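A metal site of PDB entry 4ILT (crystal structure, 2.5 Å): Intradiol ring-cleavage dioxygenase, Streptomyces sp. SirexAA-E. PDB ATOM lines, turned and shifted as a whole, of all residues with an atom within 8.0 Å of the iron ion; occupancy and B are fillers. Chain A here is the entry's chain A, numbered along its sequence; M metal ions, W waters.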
ATOM      1  N   MET A   8      -3.857  15.044 -32.795  1.00  0.00           N
ATOM      2  CA  MET A   8      -5.093  14.485 -32.270  1.00  0.00           C
ATOM      3  C   MET A   8      -5.020  14.144 -30.768  1.00  0.00           C
ATOM      4  O   MET A   8      -4.009  13.647 -30.269  1.00  0.00           O
ATOM      5  CB  MET A   8      -5.408  13.187 -33.010  1.00  0.00           C
ATOM      6  CG  MET A   8      -6.289  13.323 -34.238  1.00  0.00           C
ATOM      7  SD  MET A   8      -6.351  11.747 -35.133  1.00  0.00           S
ATOM      8  CE  MET A   8      -6.119  10.589 -33.786  1.00  0.00           C
ATOM      9  N   GLU A   9      -6.139  14.351 -30.086  1.00  0.00           N
ATOM     10  CA  GLU A   9      -6.343  13.876 -28.718  1.00  0.00           C
ATOM     11  C   GLU A   9      -6.394  12.348 -28.689  1.00  0.00           C
ATOM     12  O   GLU A   9      -5.978  11.719 -27.715  1.00  0.00           O
ATOM     13  CB  GLU A   9      -7.659  14.442 -28.196  1.00  0.00           C
ATOM     14  CG  GLU A   9      -7.763  14.723 -26.721  1.00  0.00           C
ATOM     15  CD  GLU A   9      -9.084  15.412 -26.383  1.00  0.00           C
ATOM     16  OE1 GLU A   9      -9.078  16.648 -26.143  1.00  0.00           O
ATOM     17  OE2 GLU A   9     -10.127  14.723 -26.367  1.00  0.00           O
ATOM     18  N   GLY A  10      -6.928  11.747 -29.747  1.00  0.00           N
ATOM     19  CA  GLY A  10      -7.162  10.330 -29.753  1.00  0.00           C
ATOM     20  C   GLY A  10      -8.424   9.995 -28.987  1.00  0.00           C
ATOM     21  O   GLY A  10      -9.090  10.899 -28.481  1.00  0.00           O
ATOM     22  N   PRO A  11      -8.775   8.687 -28.898  1.00  0.00           N
ATOM     23  CA  PRO A  11     -10.020   8.238 -28.275  1.00  0.00           C
ATOM     24  C   PRO A  11     -10.024   8.332 -26.770  1.00  0.00           C
ATOM     25  O   PRO A  11     -11.110   8.325 -26.203  1.00  0.00           O
ATOM     26  CB  PRO A  11     -10.106   6.754 -28.681  1.00  0.00           C
ATOM     27  CG  PRO A  11      -9.166   6.611 -29.830  1.00  0.00           C
ATOM     28  CD  PRO A  11      -8.063   7.582 -29.552  1.00  0.00           C
ATOM     29  N   TYR A  12      -8.866   8.382 -26.124  1.00  0.00           N
ATOM     30  CA  TYR A  12      -8.812   8.006 -24.709  1.00  0.00           C
ATOM     31  C   TYR A  12      -8.513   9.067 -23.622  1.00  0.00           C
ATOM     32  O   TYR A  12      -8.082   8.696 -22.536  1.00  0.00           O
ATOM     33  CB  TYR A  12      -7.861   6.809 -24.527  1.00  0.00           C
ATOM     34  CG  TYR A  12      -8.278   5.619 -25.377  1.00  0.00           C
ATOM     35  CD1 TYR A  12      -9.423   4.894 -25.078  1.00  0.00           C
ATOM     36  CD2 TYR A  12      -7.515   5.211 -26.470  1.00  0.00           C
ATOM     37  CE1 TYR A  12      -9.818   3.820 -25.837  1.00  0.00           C
ATOM     38  CE2 TYR A  12      -7.904   4.127 -27.242  1.00  0.00           C
ATOM     39  CZ  TYR A  12      -9.061   3.432 -26.924  1.00  0.00           C
ATOM     40  OH  TYR A  12      -9.474   2.349 -27.669  1.00  0.00           O
ATOM     41  N   PHE A  13      -8.766  10.348 -23.896  1.00  0.00           N
ATOM     42  CA  PHE A  13      -8.541  11.392 -22.878  1.00  0.00           C
ATOM     43  C   PHE A  13      -9.588  11.365 -21.767  1.00  0.00           C
ATOM     44  O   PHE A  13     -10.753  11.038 -22.014  1.00  0.00           O
ATOM     45  CB  PHE A  13      -8.508  12.794 -23.528  1.00  0.00           C
ATOM     46  CG  PHE A  13      -8.334  13.924 -22.542  1.00  0.00           C
ATOM     47  CD1 PHE A  13      -7.096  14.137 -21.916  1.00  0.00           C
ATOM     48  CD2 PHE A  13      -9.388  14.763 -22.223  1.00  0.00           C
ATOM     49  CE1 PHE A  13      -6.918  15.172 -20.983  1.00  0.00           C
ATOM     50  CE2 PHE A  13      -9.229  15.812 -21.292  1.00  0.00           C
ATOM     51  CZ  PHE A  13      -7.986  16.016 -20.679  1.00  0.00           C
ATOM     52  N   TRP A  55      -1.090  11.566 -20.415  1.00  0.00           N
ATOM     53  CA  TRP A  55      -1.838  10.307 -20.382  1.00  0.00           C
ATOM     54  C   TRP A  55      -1.355   9.351 -21.461  1.00  0.00           C
ATOM     55  O   TRP A  55      -1.033   9.766 -22.577  1.00  0.00           O
ATOM     56  CB  TRP A  55      -3.361  10.531 -20.455  1.00  0.00           C
ATOM     57  CG  TRP A  55      -3.931  10.820 -21.838  1.00  0.00           C
ATOM     58  CD1 TRP A  55      -4.496   9.924 -22.684  1.00  0.00           C
ATOM     59  CD2 TRP A  55      -4.040  12.103 -22.486  1.00  0.00           C
ATOM     60  NE1 TRP A  55      -4.922  10.551 -23.836  1.00  0.00           N
ATOM     61  CE2 TRP A  55      -4.661  11.887 -23.737  1.00  0.00           C
ATOM     62  CE3 TRP A  55      -3.649  13.408 -22.142  1.00  0.00           C
ATOM     63  CZ2 TRP A  55      -4.905  12.924 -24.631  1.00  0.00           C
ATOM     64  CZ3 TRP A  55      -3.887  14.425 -23.042  1.00  0.00           C
ATOM     65  CH2 TRP A  55      -4.514  14.184 -24.266  1.00  0.00           C
ATOM     66  N   GLN A  56      -1.344   8.071 -21.114  1.00  0.00           N
ATOM     67  CA  GLN A  56      -0.734   7.053 -21.944  1.00  0.00           C
ATOM     68  C   GLN A  56      -1.315   5.693 -21.649  1.00  0.00           C
ATOM     69  O   GLN A  56      -2.020   5.522 -20.667  1.00  0.00           O
ATOM     70  CB  GLN A  56       0.748   6.987 -21.649  1.00  0.00           C
ATOM     71  CG  GLN A  56       1.022   6.607 -20.197  1.00  0.00           C
ATOM     72  CD  GLN A  56       2.465   6.305 -19.929  1.00  0.00           C
ATOM     73  OE1 GLN A  56       3.222   7.186 -19.536  1.00  0.00           O
ATOM     74  NE2 GLN A  56       2.861   5.060 -20.118  1.00  0.00           N
ATOM     75  N   ALA A  57      -0.970   4.721 -22.474  1.00  0.00           N
ATOM     76  CA  ALA A  57      -1.353   3.331 -22.278  1.00  0.00           C
ATOM     77  C   ALA A  57      -0.473   2.725 -21.199  1.00  0.00           C
ATOM     78  O   ALA A  57       0.579   3.275 -20.866  1.00  0.00           O
ATOM     79  CB  ALA A  57      -1.178   2.577 -23.573  1.00  0.00           C
ATOM     80  N   GLY A  61      -0.343  -1.780 -23.299  1.00  0.00           N
ATOM     81  CA  GLY A  61      -0.835  -1.078 -24.460  1.00  0.00           C
ATOM     82  C   GLY A  61      -2.254  -0.631 -24.241  1.00  0.00           C
ATOM     83  O   GLY A  61      -2.982  -0.351 -25.184  1.00  0.00           O
ATOM     84  N   TYR A  63      -5.283   1.663 -22.277  1.00  0.00           N
ATOM     85  CA  TYR A  63      -5.692   2.909 -21.621  1.00  0.00           C
ATOM     86  C   TYR A  63      -6.773   2.638 -20.552  1.00  0.00           C
ATOM     87  O   TYR A  63      -7.646   1.786 -20.740  1.00  0.00           O
ATOM     88  CB  TYR A  63      -6.178   3.942 -22.664  1.00  0.00           C
ATOM     89  CG  TYR A  63      -5.069   4.520 -23.562  1.00  0.00           C
ATOM     90  CD1 TYR A  63      -4.423   5.708 -23.225  1.00  0.00           C
ATOM     91  CD2 TYR A  63      -4.700   3.890 -24.756  1.00  0.00           C
ATOM     92  CE1 TYR A  63      -3.427   6.251 -24.028  1.00  0.00           C
ATOM     93  CE2 TYR A  63      -3.706   4.423 -25.560  1.00  0.00           C
ATOM     94  CZ  TYR A  63      -3.072   5.608 -25.189  1.00  0.00           C
ATOM     95  OH  TYR A  63      -2.091   6.161 -25.975  1.00  0.00           O
ATOM     96  N   PRO A  89       5.057   3.061 -22.415  1.00  0.00           N
ATOM     97  CA  PRO A  89       3.738   2.517 -22.803  1.00  0.00           C
ATOM     98  C   PRO A  89       3.839   1.477 -23.895  1.00  0.00           C
ATOM     99  O   PRO A  89       4.803   1.475 -24.663  1.00  0.00           O
ATOM    100  CB  PRO A  89       2.968   3.759 -23.287  1.00  0.00           C
ATOM    101  CG  PRO A  89       4.008   4.694 -23.757  1.00  0.00           C
ATOM    102  CD  PRO A  89       5.229   4.464 -22.838  1.00  0.00           C
ATOM    103  N   GLY A  90       2.886   0.542 -23.921  1.00  0.00           N
ATOM    104  CA  GLY A  90       2.897  -0.516 -24.919  1.00  0.00           C
ATOM    105  C   GLY A  90       2.224  -0.062 -26.189  1.00  0.00           C
ATOM    106  O   GLY A  90       1.597   1.016 -26.248  1.00  0.00           O
ATOM    107  N   TYR A  92      -0.469   0.268 -28.548  1.00  0.00           N
ATOM    108  CA  TYR A  92      -1.896   0.168 -28.827  1.00  0.00           C
ATOM    109  C   TYR A  92      -2.056  -0.133 -30.332  1.00  0.00           C
ATOM    110  O   TYR A  92      -1.351   0.427 -31.171  1.00  0.00           O
ATOM    111  CB  TYR A  92      -2.575   1.468 -28.406  1.00  0.00           C
ATOM    112  CG  TYR A  92      -4.003   1.613 -28.805  1.00  0.00           C
ATOM    113  CD1 TYR A  92      -5.032   1.100 -28.019  1.00  0.00           C
ATOM    114  CD2 TYR A  92      -4.340   2.325 -29.941  1.00  0.00           C
ATOM    115  CE1 TYR A  92      -6.388   1.258 -28.392  1.00  0.00           C
ATOM    116  CE2 TYR A  92      -5.668   2.492 -30.329  1.00  0.00           C
ATOM    117  CZ  TYR A  92      -6.691   1.957 -29.550  1.00  0.00           C
ATOM    118  OH  TYR A  92      -7.991   2.143 -29.963  1.00  0.00           O
ATOM    119  N   ARG A  95      -1.261   2.215 -33.695  1.00  0.00           N
ATOM    120  CA  ARG A  95      -0.500   3.414 -33.365  1.00  0.00           C
ATOM    121  C   ARG A  95       0.950   3.041 -33.040  1.00  0.00           C
ATOM    122  O   ARG A  95       1.195   1.948 -32.516  1.00  0.00           O
ATOM    123  CB  ARG A  95      -1.111   4.113 -32.136  1.00  0.00           C
ATOM    124  CG  ARG A  95      -2.499   4.710 -32.316  1.00  0.00           C
ATOM    125  CD  ARG A  95      -2.503   5.874 -33.310  1.00  0.00           C
ATOM    126  NE  ARG A  95      -1.303   6.702 -33.212  1.00  0.00           N
ATOM    127  CZ  ARG A  95      -1.131   7.720 -32.365  1.00  0.00           C
ATOM    128  NH1 ARG A  95      -2.072   8.061 -31.492  1.00  0.00           N
ATOM    129  NH2 ARG A  95       0.025   8.377 -32.375  1.00  0.00           N
ATOM    130  N   THR A  96       1.890   3.934 -33.325  1.00  0.00           N
ATOM    131  CA  THR A  96       3.256   3.766 -32.841  1.00  0.00           C
ATOM    132  C   THR A  96       3.281   4.148 -31.369  1.00  0.00           C
ATOM    133  O   THR A  96       2.294   4.665 -30.848  1.00  0.00           O
ATOM    134  CB  THR A  96       4.270   4.593 -33.643  1.00  0.00           C
ATOM    135  OG1 THR A  96       5.588   4.203 -33.256  1.00  0.00           O
ATOM    136  CG2 THR A  96       4.110   6.085 -33.403  1.00  0.00           C
ATOM    137  N   ARG A  97       4.375   3.830 -30.666  1.00  0.00           N
ATOM    138  CA  ARG A  97       4.480   4.144 -29.249  1.00  0.00           C
ATOM    139  C   ARG A  97       4.413   5.658 -29.060  1.00  0.00           C
ATOM    140  O   ARG A  97       5.120   6.418 -29.732  1.00  0.00           O
ATOM    141  CB  ARG A  97       5.779   3.604 -28.677  1.00  0.00           C
ATOM    142  CG  ARG A  97       5.643   3.090 -27.271  1.00  0.00           C
ATOM    143  CD  ARG A  97       6.977   2.607 -26.643  1.00  0.00           C
ATOM    144  NE  ARG A  97       7.614   1.518 -27.379  1.00  0.00           N
ATOM    145  CZ  ARG A  97       7.180   0.260 -27.385  1.00  0.00           C
ATOM    146  NH1 ARG A  97       6.075  -0.086 -26.725  1.00  0.00           N
ATOM    147  NH2 ARG A  97       7.840  -0.641 -28.099  1.00  0.00           N
ATOM    148  N   HIS A  98       3.585   6.094 -28.134  1.00  0.00           N
ATOM    149  CA  HIS A  98       3.373   7.520 -27.935  1.00  0.00           C
ATOM    150  C   HIS A  98       2.848   7.785 -26.533  1.00  0.00           C
ATOM    151  O   HIS A  98       2.225   6.907 -25.917  1.00  0.00           O
ATOM    152  CB  HIS A  98       2.366   8.028 -28.970  1.00  0.00           C
ATOM    153  CG  HIS A  98       1.021   7.417 -28.838  1.00  0.00           C
ATOM    154  ND1 HIS A  98       0.709   6.180 -29.377  1.00  0.00           N
ATOM    155  CD2 HIS A  98      -0.110   7.855 -28.233  1.00  0.00           C
ATOM    156  CE1 HIS A  98      -0.544   5.891 -29.109  1.00  0.00           C
ATOM    157  NE2 HIS A  98      -1.070   6.895 -28.420  1.00  0.00           N
ATOM    158  N   ILE A  99       3.090   9.001 -26.043  1.00  0.00           N
ATOM    159  CA  ILE A  99       2.478   9.524 -24.807  1.00  0.00           C
ATOM    160  C   ILE A  99       1.720  10.806 -25.159  1.00  0.00           C
ATOM    161  O   ILE A  99       2.219  11.639 -25.931  1.00  0.00           O
ATOM    162  CB  ILE A  99       3.538   9.864 -23.729  1.00  0.00           C
ATOM    163  CG1 ILE A  99       4.206   8.583 -23.217  1.00  0.00           C
ATOM    164  CG2 ILE A  99       2.911  10.624 -22.547  1.00  0.00           C
ATOM    165  CD1 ILE A  99       5.338   8.823 -22.241  1.00  0.00           C
ATOM    166  N   HIS A 100       0.499  10.958 -24.662  1.00  0.00           N
ATOM    167  CA  HIS A 100      -0.273  12.166 -24.920  1.00  0.00           C
ATOM    168  C   HIS A 100      -0.012  13.239 -23.864  1.00  0.00           C
ATOM    169  O   HIS A 100       0.257  12.954 -22.686  1.00  0.00           O
ATOM    170  CB  HIS A 100      -1.754  11.874 -24.898  1.00  0.00           C
ATOM    171  CG  HIS A 100      -2.177  10.817 -25.867  1.00  0.00           C
ATOM    172  ND1 HIS A 100      -2.714  11.119 -27.109  1.00  0.00           N
ATOM    173  CD2 HIS A 100      -2.184   9.467 -25.772  1.00  0.00           C
ATOM    174  CE1 HIS A 100      -3.005   9.995 -27.736  1.00  0.00           C
ATOM    175  NE2 HIS A 100      -2.701   8.982 -26.937  1.00  0.00           N
ATOM    176  N   GLN A 114       1.317  14.938 -28.889  1.00  0.00           N
ATOM    177  CA  GLN A 114       1.769  13.601 -28.552  1.00  0.00           C
ATOM    178  C   GLN A 114       3.291  13.546 -28.634  1.00  0.00           C
ATOM    179  O   GLN A 114       3.877  14.229 -29.470  1.00  0.00           O
ATOM    180  CB  GLN A 114       1.154  12.567 -29.509  1.00  0.00           C
ATOM    181  CG  GLN A 114      -0.355  12.689 -29.669  1.00  0.00           C
ATOM    182  CD  GLN A 114      -0.968  11.500 -30.363  1.00  0.00           C
ATOM    183  OE1 GLN A 114      -0.299  10.484 -30.555  1.00  0.00           O
ATOM    184  NE2 GLN A 114      -2.260  11.590 -30.702  1.00  0.00           N
ATOM    185  N   LEU A 128       0.634   9.747 -37.743  1.00  0.00           N
ATOM    186  CA  LEU A 128       0.731  10.794 -36.733  1.00  0.00           C
ATOM    187  C   LEU A 128       2.169  11.060 -36.275  1.00  0.00           C
ATOM    188  O   LEU A 128       2.444  12.085 -35.653  1.00  0.00           O
ATOM    189  CB  LEU A 128      -0.121  10.477 -35.501  1.00  0.00           C
ATOM    190  CG  LEU A 128      -1.632  10.620 -35.530  1.00  0.00           C
ATOM    191  CD1 LEU A 128      -2.157  10.351 -34.131  1.00  0.00           C
ATOM    192  CD2 LEU A 128      -2.026  12.005 -35.977  1.00  0.00           C
HETATM  193 FE    FE M   1      -2.776   7.091 -27.513  1.00  0.00          FE
HETATM  194  O   HOH W   1      -4.454   7.081 -28.668  1.00  0.00           O
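Within 4 Å of the iron ion: Tyr 63, His 98 and His 100. Along chain A the residues within 4 Å of the iron ion span positions 63 to 100. The nearest printed residue that does not touch the iron ion is Arg 95 (4.2 Å).
ND1 of His 100 is in hydrogen-bond range of O of Glu 9 (3.4 Å). O of Thr 96 sits at hydrogen-bond distance from ND1 of His 98 (2.6 Å). NE2 of His 98 lies close to NH1 of Arg 95 (3.4 Å). The backbone NH (N) of His 100 is in hydrogen-bond range of the backbone carbonyl oxygen (O) of Trp 55, 2.8 Å away.
The iron ion is bound by OH of Tyr 63 (1.9 Å), NE2 of His 98 (1.9 Å), NE2 of His 100 (2.0 Å) and water W1 (2.0 Å).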
